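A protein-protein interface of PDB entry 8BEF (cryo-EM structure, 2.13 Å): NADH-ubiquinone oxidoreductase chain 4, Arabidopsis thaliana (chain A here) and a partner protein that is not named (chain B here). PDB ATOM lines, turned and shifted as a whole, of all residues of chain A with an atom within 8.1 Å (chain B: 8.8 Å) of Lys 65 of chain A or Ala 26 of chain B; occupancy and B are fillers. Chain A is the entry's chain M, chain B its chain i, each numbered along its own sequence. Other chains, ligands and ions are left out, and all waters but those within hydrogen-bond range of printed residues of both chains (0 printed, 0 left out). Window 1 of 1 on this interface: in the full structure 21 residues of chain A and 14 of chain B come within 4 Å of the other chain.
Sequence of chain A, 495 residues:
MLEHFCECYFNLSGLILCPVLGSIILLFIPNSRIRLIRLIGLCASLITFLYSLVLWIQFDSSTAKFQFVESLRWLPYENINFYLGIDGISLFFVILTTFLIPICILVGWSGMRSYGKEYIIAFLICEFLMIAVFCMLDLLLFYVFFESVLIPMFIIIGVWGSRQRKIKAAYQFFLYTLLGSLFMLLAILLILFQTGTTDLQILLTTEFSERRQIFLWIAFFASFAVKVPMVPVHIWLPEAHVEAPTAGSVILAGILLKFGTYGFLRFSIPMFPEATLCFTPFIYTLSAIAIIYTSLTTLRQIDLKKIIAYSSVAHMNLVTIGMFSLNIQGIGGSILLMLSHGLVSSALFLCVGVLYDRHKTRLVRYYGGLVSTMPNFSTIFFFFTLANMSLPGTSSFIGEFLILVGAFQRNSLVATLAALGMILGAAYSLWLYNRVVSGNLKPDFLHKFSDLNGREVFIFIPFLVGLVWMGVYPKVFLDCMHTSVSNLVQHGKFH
Of the 16 printed residues of chain B, 9 touch a printed residue of chain A. Hydrophobic or aromatic side chains of chain B that line the printed part of chain A: Ala 26, His 29 and Met 33. Printed residues of chain A that touch a printed residue of chain B: Leu 2, His 4, Asp 60, Lys 65, Phe 66, Gln 67, Phe 68 and Ile 202. Hydrophobic or aromatic side chains of chain A within 4 Å of the printed part of chain B: Leu 2, His 4, Phe 68 and Ile 202. Among the printed residues, 12 pairs touch across the chains. Among the printed residues, Asp or Glu carboxylates within 4 Å of a Lys or Arg side-chain nitrogen of the other chain: Asp 60 of chain A with Arg 22 of chain B and Lys 65 of chain A with Asp 23 of chain B.
The side-chain carboxylate (OE2) of Glu 17 of chain B sits at hydrogen-bond distance from the backbone NH (N) of Phe 68 of chain A, at 2.5 Å. NH1 of Arg 22 of chain B is in salt-bridge range of OD2 of Asp 60 of chain A. The side-chain carboxylate (OD1) of Asp 23 of chain B lies within salt-bridge range of the side-chain amino group (NZ) of Lys 65 of chain A (3.3 Å).
Among the printed residues, merely in contact across the chains: Gln 67 of chain A with Glu 17 of chain B (3.3 Å), Ile 202 of chain A with Met 33 of chain B (3.5 Å), His 4 of chain A with Lys 25 of chain B (3.6 Å), Leu 2 of chain A with His 29 of chain B (3.6 Å), Ile 202 of chain A with His 29 of chain B (3.6 Å), Leu 2 of chain A with Glu 32 of chain B (3.7 Å), Leu 2 of chain A with Glu 28 of chain B (3.8 Å), Lys 65 of chain A with Ala 26 of chain B (3.9 Å) and Phe 66 of chain A with Arg 22 of chain B (3.98 Å).
Lys 65 of chain A touches just these residues of chain B: Asp 23 and Ala 26. Printed residues of chain A within 4 Å of Ala 26 of chain B: Lys 65. No residue of chain B comes within 4 Å of Ala 64 of chain A. Printed residues of chain B within 4 Å of Phe 66 of chain A: Arg 22. Of the printed residues of chain A, Glu 17 of chain B touches Gln 67 (3.3 Å) and Phe 68 (2.5 Å). Of the printed residues of chain A, Met 33 of chain B touches Ile 202. Ile 30 of chain B touches none of the printed residues of chain A. Gly 88 of chain A touches none of the printed residues of chain B. The nearest printed residue of chain A that does not touch Ala 26 of chain B is His 4 of chain A (4.002 Å).
O of Pro 19 of chain B lies within hydrogen-bond range of NH1 of Arg 22 of chain B. The side-chain carboxylate of Asp 23 of chain B is in salt-bridge range of the guanidinium group of Arg 22 of chain B (3.0 Å). OE1 of Glu 28 of chain B is in salt-bridge range of NH1 of Arg 24 of chain B (3.4 Å). OD1 of Asp 60 of chain A sits at hydrogen-bond distance from OG of Ser 62 of chain A (2.8 Å). OG1 of Thr 63 of chain A is in hydrogen-bond range of N of Lys 65 of chain A, 2.7 Å away. N of Gln 67 of chain A is in hydrogen-bond range of O of Ile 86 of chain A.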
ATOM      1  N   LEU A   2       0.141  19.178  -2.229  1.00  0.00           N
ATOM      2  CA  LEU A   2       0.080  20.609  -1.845  1.00  0.00           C
ATOM      3  C   LEU A   2      -1.366  20.940  -1.469  1.00  0.00           C
ATOM      4  O   LEU A   2      -2.246  20.782  -2.334  1.00  0.00           O
ATOM      5  CB  LEU A   2       0.574  21.457  -3.027  1.00  0.00           C
ATOM      6  CG  LEU A   2       0.908  22.913  -2.705  1.00  0.00           C
ATOM      7  CD1 LEU A   2       2.127  22.987  -1.799  1.00  0.00           C
ATOM      8  CD2 LEU A   2       1.148  23.711  -3.980  1.00  0.00           C
ATOM      9  N   HIS A   4      -4.227  23.219  -1.254  1.00  0.00           N
ATOM     10  CA  HIS A   4      -4.638  24.457  -1.902  1.00  0.00           C
ATOM     11  C   HIS A   4      -5.885  25.051  -1.255  1.00  0.00           C
ATOM     12  O   HIS A   4      -6.707  25.665  -1.942  1.00  0.00           O
ATOM     13  CB  HIS A   4      -4.872  24.195  -3.390  1.00  0.00           C
ATOM     14  CG  HIS A   4      -4.580  25.364  -4.277  1.00  0.00           C
ATOM     15  ND1 HIS A   4      -3.955  25.229  -5.497  1.00  0.00           N
ATOM     16  CD2 HIS A   4      -4.855  26.683  -4.139  1.00  0.00           C
ATOM     17  CE1 HIS A   4      -3.842  26.416  -6.065  1.00  0.00           C
ATOM     18  NE2 HIS A   4      -4.383  27.314  -5.263  1.00  0.00           N
ATOM     19  N   PHE A  59     -17.241  36.404  -6.673  1.00  0.00           N
ATOM     20  CA  PHE A  59     -16.462  36.110  -7.868  1.00  0.00           C
ATOM     21  C   PHE A  59     -15.595  37.305  -8.243  1.00  0.00           C
ATOM     22  O   PHE A  59     -16.022  38.456  -8.131  1.00  0.00           O
ATOM     23  CB  PHE A  59     -17.387  35.745  -9.029  1.00  0.00           C
ATOM     24  CG  PHE A  59     -16.668  35.230 -10.243  1.00  0.00           C
ATOM     25  CD1 PHE A  59     -16.123  33.956 -10.255  1.00  0.00           C
ATOM     26  CD2 PHE A  59     -16.549  36.014 -11.376  1.00  0.00           C
ATOM     27  CE1 PHE A  59     -15.468  33.477 -11.375  1.00  0.00           C
ATOM     28  CE2 PHE A  59     -15.891  35.544 -12.496  1.00  0.00           C
ATOM     29  CZ  PHE A  59     -15.352  34.275 -12.497  1.00  0.00           C
ATOM     30  N   ASP A  60     -14.372  37.028  -8.692  1.00  0.00           N
ATOM     31  CA  ASP A  60     -13.417  38.064  -9.077  1.00  0.00           C
ATOM     32  C   ASP A  60     -13.286  38.007 -10.597  1.00  0.00           C
ATOM     33  O   ASP A  60     -12.735  37.047 -11.145  1.00  0.00           O
ATOM     34  CB  ASP A  60     -12.078  37.850  -8.365  1.00  0.00           C
ATOM     35  CG  ASP A  60     -10.888  38.459  -9.107  1.00  0.00           C
ATOM     36  OD1 ASP A  60     -11.062  39.420  -9.886  1.00  0.00           O
ATOM     37  OD2 ASP A  60      -9.763  37.964  -8.903  1.00  0.00           O
ATOM     38  N   SER A  62     -11.567  39.703 -12.839  1.00  0.00           N
ATOM     39  CA  SER A  62     -10.393  40.274 -13.482  1.00  0.00           C
ATOM     40  C   SER A  62      -9.300  39.260 -13.778  1.00  0.00           C
ATOM     41  O   SER A  62      -8.440  39.535 -14.620  1.00  0.00           O
ATOM     42  CB  SER A  62      -9.800  41.391 -12.612  1.00  0.00           C
ATOM     43  OG  SER A  62      -9.190  40.852 -11.455  1.00  0.00           O
ATOM     44  N   THR A  63      -9.312  38.109 -13.119  1.00  0.00           N
ATOM     45  CA  THR A  63      -8.238  37.140 -13.249  1.00  0.00           C
ATOM     46  C   THR A  63      -8.563  36.109 -14.321  1.00  0.00           C
ATOM     47  O   THR A  63      -9.727  35.786 -14.572  1.00  0.00           O
ATOM     48  CB  THR A  63      -7.986  36.433 -11.917  1.00  0.00           C
ATOM     49  OG1 THR A  63      -7.131  35.307 -12.129  1.00  0.00           O
ATOM     50  CG2 THR A  63      -9.296  35.946 -11.327  1.00  0.00           C
ATOM     51  N   ALA A  64      -7.516  35.602 -14.965  1.00  0.00           N
ATOM     52  CA  ALA A  64      -7.650  34.455 -15.847  1.00  0.00           C
ATOM     53  C   ALA A  64      -7.476  33.134 -15.112  1.00  0.00           C
ATOM     54  O   ALA A  64      -7.686  32.075 -15.714  1.00  0.00           O
ATOM     55  CB  ALA A  64      -6.636  34.545 -16.993  1.00  0.00           C
ATOM     56  N   LYS A  65      -7.110  33.172 -13.834  1.00  0.00           N
ATOM     57  CA  LYS A  65      -6.870  31.962 -13.066  1.00  0.00           C
ATOM     58  C   LYS A  65      -8.193  31.301 -12.677  1.00  0.00           C
ATOM     59  O   LYS A  65      -9.286  31.788 -12.983  1.00  0.00           O
ATOM     60  CB  LYS A  65      -6.055  32.281 -11.814  1.00  0.00           C
ATOM     61  CG  LYS A  65      -4.782  33.071 -12.059  1.00  0.00           C
ATOM     62  CD  LYS A  65      -3.828  32.348 -12.988  1.00  0.00           C
ATOM     63  CE  LYS A  65      -2.391  32.759 -12.702  1.00  0.00           C
ATOM     64  NZ  LYS A  65      -2.123  32.780 -11.236  1.00  0.00           N
ATOM     65  N   PHE A  66      -8.079  30.169 -11.989  1.00  0.00           N
ATOM     66  CA  PHE A  66      -9.223  29.492 -11.397  1.00  0.00           C
ATOM     67  C   PHE A  66      -9.436  30.034  -9.991  1.00  0.00           C
ATOM     68  O   PHE A  66      -8.482  30.156  -9.216  1.00  0.00           O
ATOM     69  CB  PHE A  66      -8.993  27.979 -11.356  1.00  0.00           C
ATOM     70  CG  PHE A  66      -9.001  27.324 -12.706  1.00  0.00           C
ATOM     71  CD1 PHE A  66     -10.079  27.473 -13.561  1.00  0.00           C
ATOM     72  CD2 PHE A  66      -7.922  26.570 -13.125  1.00  0.00           C
ATOM     73  CE1 PHE A  66     -10.077  26.868 -14.805  1.00  0.00           C
ATOM     74  CE2 PHE A  66      -7.917  25.970 -14.364  1.00  0.00           C
ATOM     75  CZ  PHE A  66      -8.997  26.121 -15.206  1.00  0.00           C
ATOM     76  N   GLN A  67     -10.677  30.370  -9.668  1.00  0.00           N
ATOM     77  CA  GLN A  67     -11.001  30.985  -8.390  1.00  0.00           C
ATOM     78  C   GLN A  67     -11.578  29.959  -7.422  1.00  0.00           C
ATOM     79  O   GLN A  67     -12.054  28.893  -7.816  1.00  0.00           O
ATOM     80  CB  GLN A  67     -11.983  32.144  -8.581  1.00  0.00           C
ATOM     81  CG  GLN A  67     -11.404  33.299  -9.364  1.00  0.00           C
ATOM     82  CD  GLN A  67     -12.464  34.159 -10.014  1.00  0.00           C
ATOM     83  OE1 GLN A  67     -13.306  34.746  -9.337  1.00  0.00           O
ATOM     84  NE2 GLN A  67     -12.425  34.243 -11.335  1.00  0.00           N
ATOM     85  N   PHE A  68     -11.517  30.302  -6.135  1.00  0.00           N
ATOM     86  CA  PHE A  68     -11.991  29.450  -5.042  1.00  0.00           C
ATOM     87  C   PHE A  68     -11.357  28.066  -5.081  1.00  0.00           C
ATOM     88  O   PHE A  68     -11.931  27.104  -4.563  1.00  0.00           O
ATOM     89  CB  PHE A  68     -13.521  29.329  -5.045  1.00  0.00           C
ATOM     90  CG  PHE A  68     -14.226  30.630  -5.259  1.00  0.00           C
ATOM     91  CD1 PHE A  68     -13.852  31.762  -4.552  1.00  0.00           C
ATOM     92  CD2 PHE A  68     -15.266  30.726  -6.162  1.00  0.00           C
ATOM     93  CE1 PHE A  68     -14.500  32.958  -4.752  1.00  0.00           C
ATOM     94  CE2 PHE A  68     -15.915  31.921  -6.362  1.00  0.00           C
ATOM     95  CZ  PHE A  68     -15.532  33.036  -5.656  1.00  0.00           C
ATOM     96  N   VAL A  69     -10.176  27.955  -5.694  1.00  0.00           N
ATOM     97  CA  VAL A  69      -9.523  26.660  -5.832  1.00  0.00           C
ATOM     98  C   VAL A  69      -9.307  26.037  -4.465  1.00  0.00           C
ATOM     99  O   VAL A  69      -8.746  26.659  -3.555  1.00  0.00           O
ATOM    100  CB  VAL A  69      -8.199  26.802  -6.591  1.00  0.00           C
ATOM    101  CG1 VAL A  69      -7.465  25.473  -6.626  1.00  0.00           C
ATOM    102  CG2 VAL A  69      -8.464  27.288  -7.990  1.00  0.00           C
ATOM    103  N   GLY A  85     -12.356  23.914  -8.717  1.00  0.00           N
ATOM    104  CA  GLY A  85     -12.303  25.344  -8.926  1.00  0.00           C
ATOM    105  C   GLY A  85     -13.173  25.728 -10.095  1.00  0.00           C
ATOM    106  O   GLY A  85     -13.486  24.902 -10.960  1.00  0.00           O
ATOM    107  N   ILE A  86     -13.562  26.998 -10.113  1.00  0.00           N
ATOM    108  CA  ILE A  86     -14.386  27.508 -11.198  1.00  0.00           C
ATOM    109  C   ILE A  86     -13.692  28.675 -11.885  1.00  0.00           C
ATOM    110  O   ILE A  86     -12.604  29.096 -11.477  1.00  0.00           O
ATOM    111  CB  ILE A  86     -15.803  27.874 -10.695  1.00  0.00           C
ATOM    112  CG1 ILE A  86     -15.804  28.820  -9.475  1.00  0.00           C
ATOM    113  CG2 ILE A  86     -16.592  26.607 -10.373  1.00  0.00           C
ATOM    114  CD1 ILE A  86     -15.119  30.176  -9.619  1.00  0.00           C
ATOM    115  N   ASP A  87     -14.318  29.195 -12.931  1.00  0.00           N
ATOM    116  CA  ASP A  87     -13.873  30.407 -13.601  1.00  0.00           C
ATOM    117  C   ASP A  87     -15.113  31.086 -14.170  1.00  0.00           C
ATOM    118  O   ASP A  87     -16.241  30.770 -13.777  1.00  0.00           O
ATOM    119  CB  ASP A  87     -12.811  30.085 -14.667  1.00  0.00           C
ATOM    120  CG  ASP A  87     -13.284  29.052 -15.670  1.00  0.00           C
ATOM    121  OD1 ASP A  87     -14.355  29.251 -16.274  1.00  0.00           O
ATOM    122  OD2 ASP A  87     -12.582  28.042 -15.863  1.00  0.00           O
ATOM    123  N   GLY A  88     -14.912  32.009 -15.103  1.00  0.00           N
ATOM    124  CA  GLY A  88     -16.025  32.678 -15.738  1.00  0.00           C
ATOM    125  C   GLY A  88     -16.736  31.887 -16.809  1.00  0.00           C
ATOM    126  O   GLY A  88     -17.657  32.410 -17.443  1.00  0.00           O
ATOM    127  N   LEU A 137     -11.280  20.303 -11.812  1.00  0.00           N
ATOM    128  CA  LEU A 137     -10.054  20.699 -12.492  1.00  0.00           C
ATOM    129  C   LEU A 137      -9.201  19.494 -12.869  1.00  0.00           C
ATOM    130  O   LEU A 137      -7.969  19.567 -12.835  1.00  0.00           O
ATOM    131  CB  LEU A 137      -9.257  21.654 -11.606  1.00  0.00           C
ATOM    132  CG  LEU A 137      -9.860  23.030 -11.332  1.00  0.00           C
ATOM    133  CD1 LEU A 137      -8.774  23.996 -10.893  1.00  0.00           C
ATOM    134  CD2 LEU A 137     -10.592  23.560 -12.554  1.00  0.00           C
ATOM    135  N   GLN A 201      -4.697  22.016 -14.775  1.00  0.00           N
ATOM    136  CA  GLN A 201      -3.788  23.157 -14.801  1.00  0.00           C
ATOM    137  C   GLN A 201      -2.456  22.786 -15.441  1.00  0.00           C
ATOM    138  O   GLN A 201      -1.901  23.560 -16.229  1.00  0.00           O
ATOM    139  CB  GLN A 201      -3.589  23.682 -13.378  1.00  0.00           C
ATOM    140  CG  GLN A 201      -4.869  24.204 -12.748  1.00  0.00           C
ATOM    141  CD  GLN A 201      -4.671  24.716 -11.338  1.00  0.00           C
ATOM    142  OE1 GLN A 201      -3.893  25.641 -11.108  1.00  0.00           O
ATOM    143  NE2 GLN A 201      -5.366  24.110 -10.382  1.00  0.00           N
ATOM    144  N   ILE A 202      -1.935  21.598 -15.127  1.00  0.00           N
ATOM    145  CA  ILE A 202      -0.683  21.153 -15.732  1.00  0.00           C
ATOM    146  C   ILE A 202      -0.858  20.918 -17.230  1.00  0.00           C
ATOM    147  O   ILE A 202      -0.031  21.353 -18.039  1.00  0.00           O
ATOM    148  CB  ILE A 202      -0.154  19.897 -15.020  1.00  0.00           C
ATOM    149  CG1 ILE A 202      -0.145  20.104 -13.504  1.00  0.00           C
ATOM    150  CG2 ILE A 202       1.234  19.552 -15.517  1.00  0.00           C
ATOM    151  CD1 ILE A 202       0.532  21.388 -13.073  1.00  0.00           C
ATOM    152  N   GLU B  17     -11.602  35.975  -2.198  1.00  0.00           N
ATOM    153  CA  GLU B  17     -10.279  35.588  -1.723  1.00  0.00           C
ATOM    154  C   GLU B  17      -9.240  36.663  -2.040  1.00  0.00           C
ATOM    155  O   GLU B  17      -9.514  37.604  -2.782  1.00  0.00           O
ATOM    156  CB  GLU B  17      -9.861  34.249  -2.337  1.00  0.00           C
ATOM    157  CG  GLU B  17     -10.074  34.155  -3.839  1.00  0.00           C
ATOM    158  CD  GLU B  17      -9.937  32.734  -4.361  1.00  0.00           C
ATOM    159  OE1 GLU B  17      -9.319  31.901  -3.664  1.00  0.00           O
ATOM    160  OE2 GLU B  17     -10.448  32.451  -5.465  1.00  0.00           O
ATOM    161  N   PRO B  19      -6.247  38.159  -3.941  1.00  0.00           N
ATOM    162  CA  PRO B  19      -5.681  37.862  -5.269  1.00  0.00           C
ATOM    163  C   PRO B  19      -4.201  37.530  -5.236  1.00  0.00           C
ATOM    164  O   PRO B  19      -3.751  36.661  -5.994  1.00  0.00           O
ATOM    165  CB  PRO B  19      -5.970  39.144  -6.070  1.00  0.00           C
ATOM    166  CG  PRO B  19      -6.838  40.011  -5.176  1.00  0.00           C
ATOM    167  CD  PRO B  19      -6.550  39.588  -3.781  1.00  0.00           C
ATOM    168  N   GLU B  20      -3.431  38.183  -4.361  1.00  0.00           N
ATOM    169  CA  GLU B  20      -1.999  37.912  -4.285  1.00  0.00           C
ATOM    170  C   GLU B  20      -1.729  36.476  -3.852  1.00  0.00           C
ATOM    171  O   GLU B  20      -0.984  35.745  -4.515  1.00  0.00           O
ATOM    172  CB  GLU B  20      -1.332  38.898  -3.324  1.00  0.00           C
ATOM    173  CG  GLU B  20      -0.945  40.232  -3.947  1.00  0.00           C
ATOM    174  CD  GLU B  20      -0.377  40.092  -5.345  1.00  0.00           C
ATOM    175  OE1 GLU B  20       0.853  39.919  -5.472  1.00  0.00           O
ATOM    176  OE2 GLU B  20      -1.154  40.177  -6.321  1.00  0.00           O
ATOM    177  N   GLU B  21      -2.334  36.051  -2.740  1.00  0.00           N
ATOM    178  CA  GLU B  21      -2.118  34.690  -2.258  1.00  0.00           C
ATOM    179  C   GLU B  21      -2.697  33.657  -3.218  1.00  0.00           C
ATOM    180  O   GLU B  21      -2.112  32.586  -3.410  1.00  0.00           O
ATOM    181  CB  GLU B  21      -2.717  34.523  -0.862  1.00  0.00           C
ATOM    182  CG  GLU B  21      -1.999  35.313   0.222  1.00  0.00           C
ATOM    183  CD  GLU B  21      -2.819  35.445   1.489  1.00  0.00           C
ATOM    184  OE1 GLU B  21      -3.745  34.630   1.686  1.00  0.00           O
ATOM    185  OE2 GLU B  21      -2.538  36.362   2.290  1.00  0.00           O
ATOM    186  N   ARG B  22      -3.849  33.953  -3.822  1.00  0.00           N
ATOM    187  CA  ARG B  22      -4.451  33.017  -4.766  1.00  0.00           C
ATOM    188  C   ARG B  22      -3.544  32.794  -5.974  1.00  0.00           C
ATOM    189  O   ARG B  22      -3.294  31.649  -6.380  1.00  0.00           O
ATOM    190  CB  ARG B  22      -5.822  33.532  -5.197  1.00  0.00           C
ATOM    191  CG  ARG B  22      -6.565  32.624  -6.147  1.00  0.00           C
ATOM    192  CD  ARG B  22      -6.811  33.319  -7.471  1.00  0.00           C
ATOM    193  NE  ARG B  22      -7.783  34.399  -7.341  1.00  0.00           N
ATOM    194  CZ  ARG B  22      -7.532  35.668  -7.632  1.00  0.00           C
ATOM    195  NH1 ARG B  22      -6.355  36.048  -8.099  1.00  0.00           N
ATOM    196  NH2 ARG B  22      -8.488  36.576  -7.456  1.00  0.00           N
ATOM    197  N   ASP B  23      -3.022  33.881  -6.551  1.00  0.00           N
ATOM    198  CA  ASP B  23      -2.107  33.743  -7.680  1.00  0.00           C
ATOM    199  C   ASP B  23      -0.799  33.086  -7.264  1.00  0.00           C
ATOM    200  O   ASP B  23      -0.212  32.323  -8.042  1.00  0.00           O
ATOM    201  CB  ASP B  23      -1.848  35.107  -8.314  1.00  0.00           C
ATOM    202  CG  ASP B  23      -3.057  35.639  -9.060  1.00  0.00           C
ATOM    203  OD1 ASP B  23      -3.962  34.839  -9.370  1.00  0.00           O
ATOM    204  OD2 ASP B  23      -3.102  36.856  -9.336  1.00  0.00           O
ATOM    205  N   ARG B  24      -0.252  33.136  -6.008  1.00  0.00           N
ATOM    206  CA  ARG B  24       1.011  32.457  -5.477  1.00  0.00           C
ATOM    207  C   ARG B  24       0.974  30.906  -5.176  1.00  0.00           C
ATOM    208  O   ARG B  24       1.935  30.193  -5.521  1.00  0.00           O
ATOM    209  CB  ARG B  24       1.554  32.989  -4.146  1.00  0.00           C
ATOM    210  CG  ARG B  24       2.926  32.430  -3.807  1.00  0.00           C
ATOM    211  CD  ARG B  24       3.537  32.672  -2.446  1.00  0.00           C
ATOM    212  NE  ARG B  24       2.675  32.435  -1.310  1.00  0.00           N
ATOM    213  CZ  ARG B  24       2.255  31.247  -0.914  1.00  0.00           C
ATOM    214  NH1 ARG B  24       2.600  30.158  -1.579  1.00  0.00           N
ATOM    215  NH2 ARG B  24       1.465  31.158   0.135  1.00  0.00           N
ATOM    216  N   LYS B  25      -0.051  30.387  -4.498  1.00  0.00           N
ATOM    217  CA  LYS B  25      -0.233  28.908  -4.421  1.00  0.00           C
ATOM    218  C   LYS B  25      -0.375  28.327  -5.848  1.00  0.00           C
ATOM    219  O   LYS B  25       0.092  27.235  -6.073  1.00  0.00           O
ATOM    220  CB  LYS B  25      -1.412  28.581  -3.510  1.00  0.00           C
ATOM    221  CG  LYS B  25      -1.268  28.886  -2.036  1.00  0.00           C
ATOM    222  CD  LYS B  25      -2.566  28.623  -1.326  1.00  0.00           C
ATOM    223  CE  LYS B  25      -3.644  29.633  -1.645  1.00  0.00           C
ATOM    224  NZ  LYS B  25      -5.001  29.060  -1.505  1.00  0.00           N
ATOM    225  N   ALA B  26      -0.934  29.067  -6.796  1.00  0.00           N
ATOM    226  CA  ALA B  26      -1.063  28.659  -8.211  1.00  0.00           C
ATOM    227  C   ALA B  26       0.339  28.404  -8.816  1.00  0.00           C
ATOM    228  O   ALA B  26       0.519  27.394  -9.516  1.00  0.00           O
ATOM    229  CB  ALA B  26      -1.879  29.657  -8.984  1.00  0.00           C
ATOM    230  N   ARG B  27       1.311  29.214  -8.479  1.00  0.00           N
ATOM    231  CA  ARG B  27       2.696  29.039  -8.971  1.00  0.00           C
ATOM    232  C   ARG B  27       3.377  27.821  -8.298  1.00  0.00           C
ATOM    233  O   ARG B  27       3.980  27.049  -8.973  1.00  0.00           O
ATOM    234  CB  ARG B  27       3.445  30.361  -8.870  1.00  0.00           C
ATOM    235  CG  ARG B  27       2.918  31.434  -9.816  1.00  0.00           C
ATOM    236  CD  ARG B  27       3.814  32.644  -9.978  1.00  0.00           C
ATOM    237  NE  ARG B  27       4.128  33.167  -8.659  1.00  0.00           N
ATOM    238  CZ  ARG B  27       3.442  34.106  -8.028  1.00  0.00           C
ATOM    239  NH1 ARG B  27       2.401  34.685  -8.601  1.00  0.00           N
ATOM    240  NH2 ARG B  27       3.809  34.461  -6.815  1.00  0.00           N
ATOM    241  N   GLU B  28       3.137  27.638  -7.015  1.00  0.00           N
ATOM    242  CA  GLU B  28       3.768  26.513  -6.279  1.00  0.00           C
ATOM    243  C   GLU B  28       3.272  25.164  -6.842  1.00  0.00           C
ATOM    244  O   GLU B  28       4.100  24.363  -7.126  1.00  0.00           O
ATOM    245  CB  GLU B  28       3.623  26.772  -4.805  1.00  0.00           C
ATOM    246  CG  GLU B  28       4.339  25.740  -3.952  1.00  0.00           C
ATOM    247  CD  GLU B  28       4.383  26.041  -2.465  1.00  0.00           C
ATOM    248  OE1 GLU B  28       3.679  26.967  -2.026  1.00  0.00           O
ATOM    249  OE2 GLU B  28       5.126  25.345  -1.751  1.00  0.00           O
ATOM    250  N   HIS B  29       1.995  25.051  -7.174  1.00  0.00           N
ATOM    251  CA  HIS B  29       1.405  23.821  -7.748  1.00  0.00           C
ATOM    252  C   HIS B  29       2.119  23.429  -9.037  1.00  0.00           C
ATOM    253  O   HIS B  29       2.614  22.383  -9.054  1.00  0.00           O
ATOM    254  CB  HIS B  29      -0.114  24.007  -7.850  1.00  0.00           C
ATOM    255  CG  HIS B  29      -0.814  23.014  -8.710  1.00  0.00           C
ATOM    256  ND1 HIS B  29      -1.527  21.973  -8.191  1.00  0.00           N
ATOM    257  CD2 HIS B  29      -0.922  22.912 -10.048  1.00  0.00           C
ATOM    258  CE1 HIS B  29      -2.048  21.271  -9.164  1.00  0.00           C
ATOM    259  NE2 HIS B  29      -1.686  21.822 -10.310  1.00  0.00           N
ATOM    260  N   ILE B  30       2.215  24.317  -9.995  1.00  0.00           N
ATOM    261  CA  ILE B  30       2.929  24.088 -11.270  1.00  0.00           C
ATOM    262  C   ILE B  30       4.416  23.833 -11.078  1.00  0.00           C
ATOM    263  O   ILE B  30       4.906  22.925 -11.677  1.00  0.00           O
ATOM    264  CB  ILE B  30       2.709  25.291 -12.221  1.00  0.00           C
ATOM    265  CG1 ILE B  30       1.260  25.391 -12.692  1.00  0.00           C
ATOM    266  CG2 ILE B  30       3.669  25.242 -13.395  1.00  0.00           C
ATOM    267  CD1 ILE B  30       0.879  26.790 -13.120  1.00  0.00           C
ATOM    268  N   TYR B  31       5.086  24.644 -10.273  1.00  0.00           N
ATOM    269  CA  TYR B  31       6.551  24.513 -10.176  1.00  0.00           C
ATOM    270  C   TYR B  31       6.767  23.175  -9.507  1.00  0.00           C
ATOM    271  O   TYR B  31       7.544  22.372  -9.976  1.00  0.00           O
ATOM    272  CB  TYR B  31       7.194  25.655  -9.396  1.00  0.00           C
ATOM    273  CG  TYR B  31       8.668  25.538  -9.156  1.00  0.00           C
ATOM    274  CD1 TYR B  31       9.569  25.650 -10.194  1.00  0.00           C
ATOM    275  CD2 TYR B  31       9.162  25.373  -7.879  1.00  0.00           C
ATOM    276  CE1 TYR B  31      10.933  25.583  -9.974  1.00  0.00           C
ATOM    277  CE2 TYR B  31      10.523  25.312  -7.639  1.00  0.00           C
ATOM    278  CZ  TYR B  31      11.410  25.405  -8.690  1.00  0.00           C
ATOM    279  OH  TYR B  31      12.753  25.320  -8.460  1.00  0.00           O
ATOM    280  N   GLU B  32       5.922  22.931  -8.546  1.00  0.00           N
ATOM    281  CA  GLU B  32       6.009  21.612  -7.915  1.00  0.00           C
ATOM    282  C   GLU B  32       5.386  20.573  -8.828  1.00  0.00           C
ATOM    283  O   GLU B  32       5.774  19.476  -8.722  1.00  0.00           O
ATOM    284  CB  GLU B  32       5.424  21.558  -6.513  1.00  0.00           C
ATOM    285  CG  GLU B  32       5.882  20.366  -5.689  1.00  0.00           C
ATOM    286  CD  GLU B  32       5.137  20.144  -4.382  1.00  0.00           C
ATOM    287  OE1 GLU B  32       4.172  20.884  -4.112  1.00  0.00           O
ATOM    288  OE2 GLU B  32       5.525  19.221  -3.636  1.00  0.00           O
ATOM    289  N   MET B  33       4.539  20.987  -9.828  1.00  0.00           N
ATOM    290  CA  MET B  33       4.164  19.720 -10.450  1.00  0.00           C
ATOM    291  C   MET B  33       5.034  19.392 -11.659  1.00  0.00           C
ATOM    292  O   MET B  33       5.260  18.210 -11.952  1.00  0.00           O
ATOM    293  CB  MET B  33       2.683  19.732 -10.819  1.00  0.00           C
ATOM    294  CG  MET B  33       1.781  19.787  -9.600  1.00  0.00           C
ATOM    295  SD  MET B  33       2.042  18.363  -8.525  1.00  0.00           S
ATOM    296  CE  MET B  33       1.435  17.024  -9.541  1.00  0.00           C
